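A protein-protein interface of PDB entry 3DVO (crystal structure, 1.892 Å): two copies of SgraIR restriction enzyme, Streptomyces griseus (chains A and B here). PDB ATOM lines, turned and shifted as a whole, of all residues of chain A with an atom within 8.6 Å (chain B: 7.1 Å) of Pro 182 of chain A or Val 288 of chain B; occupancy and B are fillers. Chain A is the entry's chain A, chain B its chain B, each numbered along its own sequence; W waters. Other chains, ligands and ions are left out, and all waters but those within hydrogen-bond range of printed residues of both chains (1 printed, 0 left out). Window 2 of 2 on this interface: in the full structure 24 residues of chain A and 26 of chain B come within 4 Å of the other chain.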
ATOM      1  N   ASP A 154     -28.118  -4.110 -17.307  1.00  0.00           N
ATOM      2  CA  ASP A 154     -27.532  -5.349 -16.794  1.00  0.00           C
ATOM      3  C   ASP A 154     -26.927  -5.055 -15.412  1.00  0.00           C
ATOM      4  O   ASP A 154     -25.883  -4.415 -15.303  1.00  0.00           O
ATOM      5  CB  ASP A 154     -26.443  -5.852 -17.743  1.00  0.00           C
ATOM      6  CG  ASP A 154     -25.786  -7.149 -17.259  1.00  0.00           C
ATOM      7  OD1 ASP A 154     -25.952  -7.501 -16.074  1.00  0.00           O
ATOM      8  OD2 ASP A 154     -25.104  -7.823 -18.065  1.00  0.00           O
ATOM      9  N   TRP A 155     -27.582  -5.505 -14.352  1.00  0.00           N
ATOM     10  CA  TRP A 155     -27.140  -5.146 -13.026  1.00  0.00           C
ATOM     11  C   TRP A 155     -25.633  -5.394 -12.796  1.00  0.00           C
ATOM     12  O   TRP A 155     -25.025  -4.757 -11.931  1.00  0.00           O
ATOM     13  CB  TRP A 155     -27.996  -5.830 -11.947  1.00  0.00           C
ATOM     14  CG  TRP A 155     -27.860  -7.301 -11.883  1.00  0.00           C
ATOM     15  CD1 TRP A 155     -28.703  -8.223 -12.425  1.00  0.00           C
ATOM     16  CD2 TRP A 155     -26.835  -8.047 -11.190  1.00  0.00           C
ATOM     17  NE1 TRP A 155     -28.266  -9.492 -12.132  1.00  0.00           N
ATOM     18  CE2 TRP A 155     -27.114  -9.417 -11.390  1.00  0.00           C
ATOM     19  CE3 TRP A 155     -25.701  -7.692 -10.458  1.00  0.00           C
ATOM     20  CZ2 TRP A 155     -26.306 -10.438 -10.862  1.00  0.00           C
ATOM     21  CZ3 TRP A 155     -24.898  -8.710  -9.921  1.00  0.00           C
ATOM     22  CH2 TRP A 155     -25.204 -10.067 -10.137  1.00  0.00           C
ATOM     23  N   VAL A 156     -25.017  -6.265 -13.585  1.00  0.00           N
ATOM     24  CA  VAL A 156     -23.596  -6.573 -13.354  1.00  0.00           C
ATOM     25  C   VAL A 156     -22.724  -5.330 -13.527  1.00  0.00           C
ATOM     26  O   VAL A 156     -21.618  -5.240 -12.982  1.00  0.00           O
ATOM     27  CB  VAL A 156     -23.070  -7.709 -14.272  1.00  0.00           C
ATOM     28  CG1 VAL A 156     -21.568  -7.917 -14.077  1.00  0.00           C
ATOM     29  CG2 VAL A 156     -23.810  -8.990 -14.000  1.00  0.00           C
ATOM     30  N   ILE A 167     -16.980 -12.512 -12.822  1.00  0.00           N
ATOM     31  CA  ILE A 167     -18.196 -12.972 -13.468  1.00  0.00           C
ATOM     32  C   ILE A 167     -17.971 -13.192 -14.959  1.00  0.00           C
ATOM     33  O   ILE A 167     -18.382 -14.211 -15.498  1.00  0.00           O
ATOM     34  CB  ILE A 167     -19.358 -12.002 -13.261  1.00  0.00           C
ATOM     35  CG1 ILE A 167     -19.675 -11.894 -11.773  1.00  0.00           C
ATOM     36  CG2 ILE A 167     -20.601 -12.490 -14.010  1.00  0.00           C
ATOM     37  CD1 ILE A 167     -20.832 -10.969 -11.477  1.00  0.00           C
ATOM     38  N   GLU A 168     -17.309 -12.252 -15.626  1.00  0.00           N
ATOM     39  CA  GLU A 168     -17.141 -12.383 -17.069  1.00  0.00           C
ATOM     40  C   GLU A 168     -16.225 -13.541 -17.451  1.00  0.00           C
ATOM     41  O   GLU A 168     -16.411 -14.161 -18.497  1.00  0.00           O
ATOM     42  CB  GLU A 168     -16.652 -11.090 -17.707  1.00  0.00           C
ATOM     43  CG  GLU A 168     -16.643 -11.165 -19.217  1.00  0.00           C
ATOM     44  CD  GLU A 168     -18.041 -11.351 -19.806  1.00  0.00           C
ATOM     45  OE1 GLU A 168     -18.112 -11.704 -21.007  1.00  0.00           O
ATOM     46  OE2 GLU A 168     -19.056 -11.137 -19.082  1.00  0.00           O
ATOM     47  N   PHE A 170     -16.066 -16.312 -15.690  1.00  0.00           N
ATOM     48  CA  PHE A 170     -16.935 -17.452 -15.446  1.00  0.00           C
ATOM     49  C   PHE A 170     -17.855 -17.706 -16.643  1.00  0.00           C
ATOM     50  O   PHE A 170     -17.882 -18.802 -17.181  1.00  0.00           O
ATOM     51  CB  PHE A 170     -17.746 -17.218 -14.171  1.00  0.00           C
ATOM     52  CG  PHE A 170     -18.856 -18.216 -13.946  1.00  0.00           C
ATOM     53  CD1 PHE A 170     -18.573 -19.546 -13.687  1.00  0.00           C
ATOM     54  CD2 PHE A 170     -20.181 -17.811 -13.954  1.00  0.00           C
ATOM     55  CE1 PHE A 170     -19.592 -20.460 -13.463  1.00  0.00           C
ATOM     56  CE2 PHE A 170     -21.198 -18.708 -13.733  1.00  0.00           C
ATOM     57  CZ  PHE A 170     -20.906 -20.040 -13.486  1.00  0.00           C
ATOM     58  N   ARG A 171     -18.599 -16.694 -17.074  1.00  0.00           N
ATOM     59  CA  ARG A 171     -19.558 -16.914 -18.153  1.00  0.00           C
ATOM     60  C   ARG A 171     -18.906 -16.997 -19.521  1.00  0.00           C
ATOM     61  O   ARG A 171     -19.520 -17.451 -20.483  1.00  0.00           O
ATOM     62  CB  ARG A 171     -20.680 -15.863 -18.143  1.00  0.00           C
ATOM     63  CG  ARG A 171     -20.223 -14.495 -17.771  1.00  0.00           C
ATOM     64  CD  ARG A 171     -21.216 -13.419 -18.211  1.00  0.00           C
ATOM     65  NE  ARG A 171     -22.395 -13.335 -17.366  1.00  0.00           N
ATOM     66  CZ  ARG A 171     -23.080 -12.208 -17.170  1.00  0.00           C
ATOM     67  NH1 ARG A 171     -22.679 -11.072 -17.725  1.00  0.00           N
ATOM     68  NH2 ARG A 171     -24.166 -12.206 -16.420  1.00  0.00           N
ATOM     69  N   LEU A 174     -18.396 -20.551 -19.830  1.00  0.00           N
ATOM     70  CA  LEU A 174     -19.620 -21.258 -20.164  1.00  0.00           C
ATOM     71  C   LEU A 174     -19.925 -21.149 -21.653  1.00  0.00           C
ATOM     72  O   LEU A 174     -20.375 -22.118 -22.271  1.00  0.00           O
ATOM     73  CB  LEU A 174     -20.806 -20.725 -19.335  1.00  0.00           C
ATOM     74  CG  LEU A 174     -20.900 -21.019 -17.833  1.00  0.00           C
ATOM     75  CD1 LEU A 174     -22.222 -20.583 -17.308  1.00  0.00           C
ATOM     76  CD2 LEU A 174     -20.700 -22.503 -17.516  1.00  0.00           C
ATOM     77  N   ARG A 175     -19.690 -19.975 -22.228  1.00  0.00           N
ATOM     78  CA  ARG A 175     -20.040 -19.742 -23.628  1.00  0.00           C
ATOM     79  C   ARG A 175     -19.199 -20.630 -24.513  1.00  0.00           C
ATOM     80  O   ARG A 175     -19.640 -21.064 -25.566  1.00  0.00           O
ATOM     81  CB  ARG A 175     -19.851 -18.277 -24.030  1.00  0.00           C
ATOM     82  CG  ARG A 175     -20.849 -17.330 -23.423  1.00  0.00           C
ATOM     83  CD  ARG A 175     -20.723 -15.955 -24.044  1.00  0.00           C
ATOM     84  NE  ARG A 175     -20.783 -14.931 -23.017  1.00  0.00           N
ATOM     85  CZ  ARG A 175     -19.737 -14.233 -22.588  1.00  0.00           C
ATOM     86  NH1 ARG A 175     -18.537 -14.425 -23.114  1.00  0.00           N
ATOM     87  NH2 ARG A 175     -19.904 -13.327 -21.637  1.00  0.00           N
ATOM     88  N   GLY A 178     -20.952 -23.519 -25.253  1.00  0.00           N
ATOM     89  CA  GLY A 178     -22.261 -23.289 -25.843  1.00  0.00           C
ATOM     90  C   GLY A 178     -23.377 -23.053 -24.833  1.00  0.00           C
ATOM     91  O   GLY A 178     -24.557 -23.246 -25.141  1.00  0.00           O
ATOM     92  N   LEU A 179     -23.010 -22.627 -23.625  1.00  0.00           N
ATOM     93  CA  LEU A 179     -23.991 -22.306 -22.589  1.00  0.00           C
ATOM     94  C   LEU A 179     -23.964 -20.809 -22.345  1.00  0.00           C
ATOM     95  O   LEU A 179     -23.389 -20.060 -23.112  1.00  0.00           O
ATOM     96  CB  LEU A 179     -23.686 -23.054 -21.288  1.00  0.00           C
ATOM     97  CG  LEU A 179     -23.644 -24.596 -21.311  1.00  0.00           C
ATOM     98  CD1 LEU A 179     -23.166 -25.151 -19.988  1.00  0.00           C
ATOM     99  CD2 LEU A 179     -24.985 -25.198 -21.646  1.00  0.00           C
ATOM    100  N   GLY A 180     -24.594 -20.371 -21.270  1.00  0.00           N
ATOM    101  CA  GLY A 180     -24.516 -18.975 -20.888  1.00  0.00           C
ATOM    102  C   GLY A 180     -24.990 -18.786 -19.468  1.00  0.00           C
ATOM    103  O   GLY A 180     -25.305 -19.762 -18.781  1.00  0.00           O
ATOM    104  N   LEU A 181     -25.020 -17.533 -19.027  1.00  0.00           N
ATOM    105  CA  LEU A 181     -25.634 -17.174 -17.764  1.00  0.00           C
ATOM    106  C   LEU A 181     -25.911 -15.686 -17.791  1.00  0.00           C
ATOM    107  O   LEU A 181     -25.404 -14.946 -16.947  1.00  0.00           O
ATOM    108  CB  LEU A 181     -24.739 -17.541 -16.573  1.00  0.00           C
ATOM    109  CG  LEU A 181     -25.516 -17.478 -15.253  1.00  0.00           C
ATOM    110  CD1 LEU A 181     -26.739 -18.390 -15.324  1.00  0.00           C
ATOM    111  CD2 LEU A 181     -24.648 -17.827 -14.063  1.00  0.00           C
ATOM    112  N   PRO A 182     -26.705 -15.240 -18.784  1.00  0.00           N
ATOM    113  CA  PRO A 182     -27.059 -13.826 -18.916  1.00  0.00           C
ATOM    114  C   PRO A 182     -27.649 -13.270 -17.634  1.00  0.00           C
ATOM    115  O   PRO A 182     -28.193 -14.024 -16.809  1.00  0.00           O
ATOM    116  CB  PRO A 182     -28.152 -13.812 -19.997  1.00  0.00           C
ATOM    117  CG  PRO A 182     -28.092 -15.121 -20.678  1.00  0.00           C
ATOM    118  CD  PRO A 182     -27.369 -16.099 -19.779  1.00  0.00           C
ATOM    119  N   THR A 183     -27.559 -11.951 -17.487  1.00  0.00           N
ATOM    120  CA  THR A 183     -28.173 -11.231 -16.381  1.00  0.00           C
ATOM    121  C   THR A 183     -29.011 -10.097 -16.958  1.00  0.00           C
ATOM    122  O   THR A 183     -28.561  -9.387 -17.856  1.00  0.00           O
ATOM    123  CB  THR A 183     -27.096 -10.619 -15.466  1.00  0.00           C
ATOM    124  OG1 THR A 183     -26.055 -10.067 -16.278  1.00  0.00           O
ATOM    125  CG2 THR A 183     -26.510 -11.673 -14.544  1.00  0.00           C
ATOM    126  N   SER A 184     -30.227  -9.925 -16.455  1.00  0.00           N
ATOM    127  CA  SER A 184     -31.049  -8.788 -16.864  1.00  0.00           C
ATOM    128  C   SER A 184     -31.014  -7.729 -15.766  1.00  0.00           C
ATOM    129  O   SER A 184     -29.953  -7.189 -15.474  1.00  0.00           O
ATOM    130  CB  SER A 184     -32.473  -9.235 -17.163  1.00  0.00           C
ATOM    131  OG  SER A 184     -33.019  -9.907 -16.033  1.00  0.00           O
ATOM    132  N   THR A 185     -32.144  -7.432 -15.136  1.00  0.00           N
ATOM    133  CA  THR A 185     -32.135  -6.426 -14.067  1.00  0.00           C
ATOM    134  C   THR A 185     -33.424  -6.414 -13.229  1.00  0.00           C
ATOM    135  O   THR A 185     -34.477  -6.799 -13.711  1.00  0.00           O
ATOM    136  CB  THR A 185     -31.893  -5.002 -14.660  1.00  0.00           C
ATOM    137  OG1 THR A 185     -31.828  -4.031 -13.608  1.00  0.00           O
ATOM    138  CG2 THR A 185     -33.012  -4.632 -15.614  1.00  0.00           C
ATOM    139  N   TYR A 254     -36.724 -15.710 -11.246  1.00  0.00           N
ATOM    140  CA  TYR A 254     -35.575 -16.181 -11.996  1.00  0.00           C
ATOM    141  C   TYR A 254     -34.332 -15.291 -11.766  1.00  0.00           C
ATOM    142  O   TYR A 254     -33.248 -15.795 -11.473  1.00  0.00           O
ATOM    143  CB  TYR A 254     -35.878 -16.337 -13.495  1.00  0.00           C
ATOM    144  CG  TYR A 254     -34.676 -16.936 -14.167  1.00  0.00           C
ATOM    145  CD1 TYR A 254     -34.376 -18.293 -14.024  1.00  0.00           C
ATOM    146  CD2 TYR A 254     -33.774 -16.131 -14.834  1.00  0.00           C
ATOM    147  CE1 TYR A 254     -33.243 -18.833 -14.598  1.00  0.00           C
ATOM    148  CE2 TYR A 254     -32.637 -16.654 -15.406  1.00  0.00           C
ATOM    149  CZ  TYR A 254     -32.368 -17.997 -15.280  1.00  0.00           C
ATOM    150  OH  TYR A 254     -31.228 -18.479 -15.869  1.00  0.00           O
ATOM    151  N   GLU A 255     -34.489 -13.975 -11.905  1.00  0.00           N
ATOM    152  CA  GLU A 255     -33.366 -13.048 -11.739  1.00  0.00           C
ATOM    153  C   GLU A 255     -32.790 -13.053 -10.327  1.00  0.00           C
ATOM    154  O   GLU A 255     -31.567 -12.936 -10.140  1.00  0.00           O
ATOM    155  CB  GLU A 255     -33.774 -11.627 -12.137  1.00  0.00           C
ATOM    156  CG  GLU A 255     -32.592 -10.722 -12.395  1.00  0.00           C
ATOM    157  CD  GLU A 255     -31.687 -11.248 -13.509  1.00  0.00           C
ATOM    158  OE1 GLU A 255     -30.440 -11.221 -13.346  1.00  0.00           O
ATOM    159  OE2 GLU A 255     -32.229 -11.692 -14.541  1.00  0.00           O
ATOM    160  N   VAL A 258     -30.398 -15.930  -9.992  1.00  0.00           N
ATOM    161  CA  VAL A 258     -29.139 -15.715 -10.677  1.00  0.00           C
ATOM    162  C   VAL A 258     -28.262 -14.740  -9.892  1.00  0.00           C
ATOM    163  O   VAL A 258     -27.044 -14.931  -9.776  1.00  0.00           O
ATOM    164  CB  VAL A 258     -29.397 -15.207 -12.106  1.00  0.00           C
ATOM    165  CG1 VAL A 258     -28.079 -14.862 -12.806  1.00  0.00           C
ATOM    166  CG2 VAL A 258     -30.142 -16.270 -12.876  1.00  0.00           C
ATOM    167  N   MET A 259     -28.889 -13.704  -9.338  1.00  0.00           N
ATOM    168  CA  MET A 259     -28.186 -12.776  -8.463  1.00  0.00           C
ATOM    169  C   MET A 259     -27.538 -13.521  -7.300  1.00  0.00           C
ATOM    170  O   MET A 259     -26.378 -13.305  -6.987  1.00  0.00           O
ATOM    171  CB  MET A 259     -29.133 -11.697  -7.950  1.00  0.00           C
ATOM    172  CG  MET A 259     -29.547 -10.747  -9.042  1.00  0.00           C
ATOM    173  SD  MET A 259     -30.502  -9.307  -8.514  1.00  0.00           S
ATOM    174  CE  MET A 259     -29.293  -8.361  -7.597  1.00  0.00           C
ATOM    175  N   LEU A 262     -24.609 -15.699  -8.406  1.00  0.00           N
ATOM    176  CA  LEU A 262     -23.419 -14.890  -8.736  1.00  0.00           C
ATOM    177  C   LEU A 262     -22.815 -14.152  -7.536  1.00  0.00           C
ATOM    178  O   LEU A 262     -21.626 -14.291  -7.241  1.00  0.00           O
ATOM    179  CB  LEU A 262     -23.705 -13.917  -9.883  1.00  0.00           C
ATOM    180  CG  LEU A 262     -23.960 -14.593 -11.229  1.00  0.00           C
ATOM    181  CD1 LEU A 262     -24.312 -13.562 -12.304  1.00  0.00           C
ATOM    182  CD2 LEU A 262     -22.773 -15.434 -11.637  1.00  0.00           C
ATOM    183  N   TYR B 250     -39.649 -16.112 -18.788  1.00  0.00           N
ATOM    184  CA  TYR B 250     -39.049 -16.760 -17.625  1.00  0.00           C
ATOM    185  C   TYR B 250     -39.798 -17.902 -16.969  1.00  0.00           C
ATOM    186  O   TYR B 250     -39.170 -18.710 -16.281  1.00  0.00           O
ATOM    187  CB  TYR B 250     -38.596 -15.705 -16.596  1.00  0.00           C
ATOM    188  CG  TYR B 250     -37.495 -14.860 -17.177  1.00  0.00           C
ATOM    189  CD1 TYR B 250     -36.169 -15.283 -17.122  1.00  0.00           C
ATOM    190  CD2 TYR B 250     -37.784 -13.679 -17.842  1.00  0.00           C
ATOM    191  CE1 TYR B 250     -35.172 -14.547 -17.676  1.00  0.00           C
ATOM    192  CE2 TYR B 250     -36.779 -12.923 -18.396  1.00  0.00           C
ATOM    193  CZ  TYR B 250     -35.476 -13.362 -18.318  1.00  0.00           C
ATOM    194  OH  TYR B 250     -34.468 -12.606 -18.879  1.00  0.00           O
ATOM    195  N   THR B 284     -33.752 -11.233 -31.322  1.00  0.00           N
ATOM    196  CA  THR B 284     -32.752 -12.251 -31.020  1.00  0.00           C
ATOM    197  C   THR B 284     -32.525 -12.447 -29.507  1.00  0.00           C
ATOM    198  O   THR B 284     -31.903 -13.437 -29.086  1.00  0.00           O
ATOM    199  CB  THR B 284     -31.412 -11.925 -31.724  1.00  0.00           C
ATOM    200  OG1 THR B 284     -30.543 -11.229 -30.821  1.00  0.00           O
ATOM    201  CG2 THR B 284     -31.661 -11.057 -32.955  1.00  0.00           C
ATOM    202  N   ASN B 285     -33.032 -11.511 -28.699  1.00  0.00           N
ATOM    203  CA  ASN B 285     -32.886 -11.594 -27.243  1.00  0.00           C
ATOM    204  C   ASN B 285     -33.242 -12.967 -26.692  1.00  0.00           C
ATOM    205  O   ASN B 285     -32.517 -13.527 -25.864  1.00  0.00           O
ATOM    206  CB  ASN B 285     -33.766 -10.562 -26.547  1.00  0.00           C
ATOM    207  CG  ASN B 285     -33.587 -10.571 -25.025  1.00  0.00           C
ATOM    208  OD1 ASN B 285     -32.582 -10.070 -24.505  1.00  0.00           O
ATOM    209  ND2 ASN B 285     -34.561 -11.147 -24.306  1.00  0.00           N
ATOM    210  N   ALA B 286     -34.378 -13.495 -27.138  1.00  0.00           N
ATOM    211  CA  ALA B 286     -34.867 -14.766 -26.627  1.00  0.00           C
ATOM    212  C   ALA B 286     -33.896 -15.921 -26.856  1.00  0.00           C
ATOM    213  O   ALA B 286     -33.737 -16.785 -25.994  1.00  0.00           O
ATOM    214  CB  ALA B 286     -36.226 -15.090 -27.218  1.00  0.00           C
ATOM    215  N   PHE B 287     -33.256 -15.949 -28.016  1.00  0.00           N
ATOM    216  CA  PHE B 287     -32.392 -17.078 -28.328  1.00  0.00           C
ATOM    217  C   PHE B 287     -31.219 -17.063 -27.376  1.00  0.00           C
ATOM    218  O   PHE B 287     -30.847 -18.094 -26.853  1.00  0.00           O
ATOM    219  CB  PHE B 287     -31.927 -17.064 -29.790  1.00  0.00           C
ATOM    220  CG  PHE B 287     -33.041 -17.263 -30.781  1.00  0.00           C
ATOM    221  CD1 PHE B 287     -33.484 -18.537 -31.098  1.00  0.00           C
ATOM    222  CD2 PHE B 287     -33.652 -16.178 -31.381  1.00  0.00           C
ATOM    223  CE1 PHE B 287     -34.528 -18.726 -31.992  1.00  0.00           C
ATOM    224  CE2 PHE B 287     -34.683 -16.357 -32.293  1.00  0.00           C
ATOM    225  CZ  PHE B 287     -35.126 -17.622 -32.602  1.00  0.00           C
ATOM    226  N   VAL B 288     -30.655 -15.890 -27.126  1.00  0.00           N
ATOM    227  CA  VAL B 288     -29.583 -15.787 -26.144  1.00  0.00           C
ATOM    228  C   VAL B 288     -30.084 -16.089 -24.729  1.00  0.00           C
ATOM    229  O   VAL B 288     -29.413 -16.788 -23.947  1.00  0.00           O
ATOM    230  CB  VAL B 288     -28.879 -14.418 -26.187  1.00  0.00           C
ATOM    231  CG1 VAL B 288     -27.979 -14.244 -24.952  1.00  0.00           C
ATOM    232  CG2 VAL B 288     -28.065 -14.298 -27.450  1.00  0.00           C
ATOM    233  N   THR B 289     -31.266 -15.585 -24.392  1.00  0.00           N
ATOM    234  CA  THR B 289     -31.765 -15.794 -23.044  1.00  0.00           C
ATOM    235  C   THR B 289     -31.814 -17.288 -22.784  1.00  0.00           C
ATOM    236  O   THR B 289     -31.367 -17.756 -21.740  1.00  0.00           O
ATOM    237  CB  THR B 289     -33.150 -15.178 -22.813  1.00  0.00           C
ATOM    238  OG1 THR B 289     -33.083 -13.765 -23.037  1.00  0.00           O
ATOM    239  CG2 THR B 289     -33.571 -15.420 -21.386  1.00  0.00           C
ATOM    240  N   TYR B 290     -32.313 -18.045 -23.760  1.00  0.00           N
ATOM    241  CA  TYR B 290     -32.495 -19.480 -23.564  1.00  0.00           C
ATOM    242  C   TYR B 290     -31.234 -20.308 -23.725  1.00  0.00           C
ATOM    243  O   TYR B 290     -31.312 -21.531 -23.829  1.00  0.00           O
ATOM    244  CB  TYR B 290     -33.559 -20.016 -24.503  1.00  0.00           C
ATOM    245  CG  TYR B 290     -34.935 -19.613 -24.078  1.00  0.00           C
ATOM    246  CD1 TYR B 290     -35.300 -19.626 -22.735  1.00  0.00           C
ATOM    247  CD2 TYR B 290     -35.874 -19.238 -25.010  1.00  0.00           C
ATOM    248  CE1 TYR B 290     -36.572 -19.252 -22.343  1.00  0.00           C
ATOM    249  CE2 TYR B 290     -37.154 -18.877 -24.628  1.00  0.00           C
ATOM    250  CZ  TYR B 290     -37.498 -18.883 -23.301  1.00  0.00           C
ATOM    251  OH  TYR B 290     -38.782 -18.511 -22.930  1.00  0.00           O
ATOM    252  N   GLU B 291     -30.083 -19.651 -23.777  1.00  0.00           N
ATOM    253  CA  GLU B 291     -28.827 -20.393 -23.756  1.00  0.00           C
ATOM    254  C   GLU B 291     -28.375 -20.669 -22.341  1.00  0.00           C
ATOM    255  O   GLU B 291     -27.358 -21.333 -22.124  1.00  0.00           O
ATOM    256  CB  GLU B 291     -27.744 -19.645 -24.522  1.00  0.00           C
ATOM    257  CG  GLU B 291     -27.739 -19.977 -25.999  1.00  0.00           C
ATOM    258  CD  GLU B 291     -26.919 -19.008 -26.823  1.00  0.00           C
ATOM    259  OE1 GLU B 291     -26.057 -18.301 -26.238  1.00  0.00           O
ATOM    260  OE2 GLU B 291     -27.145 -18.962 -28.062  1.00  0.00           O
ATOM    261  N   ALA B 292     -29.120 -20.156 -21.373  1.00  0.00           N
ATOM    262  CA  ALA B 292     -28.684 -20.227 -19.977  1.00  0.00           C
ATOM    263  C   ALA B 292     -28.559 -21.650 -19.483  1.00  0.00           C
ATOM    264  O   ALA B 292     -29.417 -22.489 -19.755  1.00  0.00           O
ATOM    265  CB  ALA B 292     -29.643 -19.456 -19.079  1.00  0.00           C
ATOM    266  N   ALA B 293     -27.501 -21.903 -18.722  1.00  0.00           N
ATOM    267  CA  ALA B 293     -27.303 -23.194 -18.089  1.00  0.00           C
ATOM    268  C   ALA B 293     -28.223 -23.417 -16.893  1.00  0.00           C
ATOM    269  O   ALA B 293     -28.605 -22.483 -16.179  1.00  0.00           O
ATOM    270  CB  ALA B 293     -25.831 -23.372 -17.679  1.00  0.00           C
ATOM    271  N   LEU B 312     -35.099 -22.930 -28.592  1.00  0.00           N
ATOM    272  CA  LEU B 312     -36.298 -22.161 -28.959  1.00  0.00           C
ATOM    273  C   LEU B 312     -36.591 -22.491 -30.409  1.00  0.00           C
ATOM    274  O   LEU B 312     -35.761 -22.246 -31.273  1.00  0.00           O
ATOM    275  CB  LEU B 312     -36.043 -20.663 -28.806  1.00  0.00           C
ATOM    276  CG  LEU B 312     -37.180 -19.727 -29.239  1.00  0.00           C
ATOM    277  CD1 LEU B 312     -38.427 -19.996 -28.421  1.00  0.00           C
ATOM    278  CD2 LEU B 312     -36.751 -18.249 -29.149  1.00  0.00           C
HETATM  279  O   HOH W   1     -30.941 -21.240 -16.221  1.00  0.00           O
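N of Ala 293 of chain B sits at hydrogen-bond distance from O of Gly 180 of chain A, at 3.1 Å.
The backbone NH (N) of Gly 180 of chain A is in hydrogen-bond range of the backbone carbonyl oxygen (O) of Glu 291 of chain B, at 3.0 Å.
The backbone carbonyl oxygen (O) of Leu 174 of chain A is in hydrogen-bond range of the backbone NH (N) of Leu 179 of chain A, at 3.0 Å.
No position is printed for both chains.
Of the 8 pairs that touch across the chains among the printed residues, none has its exchanged pair printed and touching as well.
C of Leu 179 of chain A touches O of Glu 291 of chain B, 3.4 Å away.
Ala 293 of chain B touches Leu 179 of chain A (CB to CD1, 3.9 Å).
O of Gly 180 of chain A touches CA of Ala 292 of chain B, 3.6 Å away.
Val 288 of chain B touches Pro 182 of chain A.
CD2 of Tyr 254 of chain A touches CD1 of Tyr 250 of chain B (3.4 Å).
Ala 292 of chain B touches Tyr 254 of chain A.
Water W1 bridges the backbone carbonyl oxygen (O) of Ala 293 of chain B and the side-chain hydroxyl (OH) of Tyr 254 of chain A.
Hydrophobic or aromatic side chains of chain A within 4 Å of the printed part of chain B: Leu 179, Pro 182 and Tyr 254.
Among the printed residues, no Asp or Glu carboxylate lies within 4 Å of a Lys or Arg side-chain nitrogen of the other chain.
Printed residues of chain B within 4 Å of Gly 180 of chain A: Glu 291, Ala 292 and Ala 293.
Of the printed residues of chain A, Tyr 250 of chain B touches Tyr 254 (3.4 Å).
Of chain A, only Pro 182 (3.9 Å) comes within 4 Å of Val 288 of chain B.
The nearest printed residue of chain A that does not touch Ala 293 of chain B is Leu 174 of chain A (4.6 Å).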
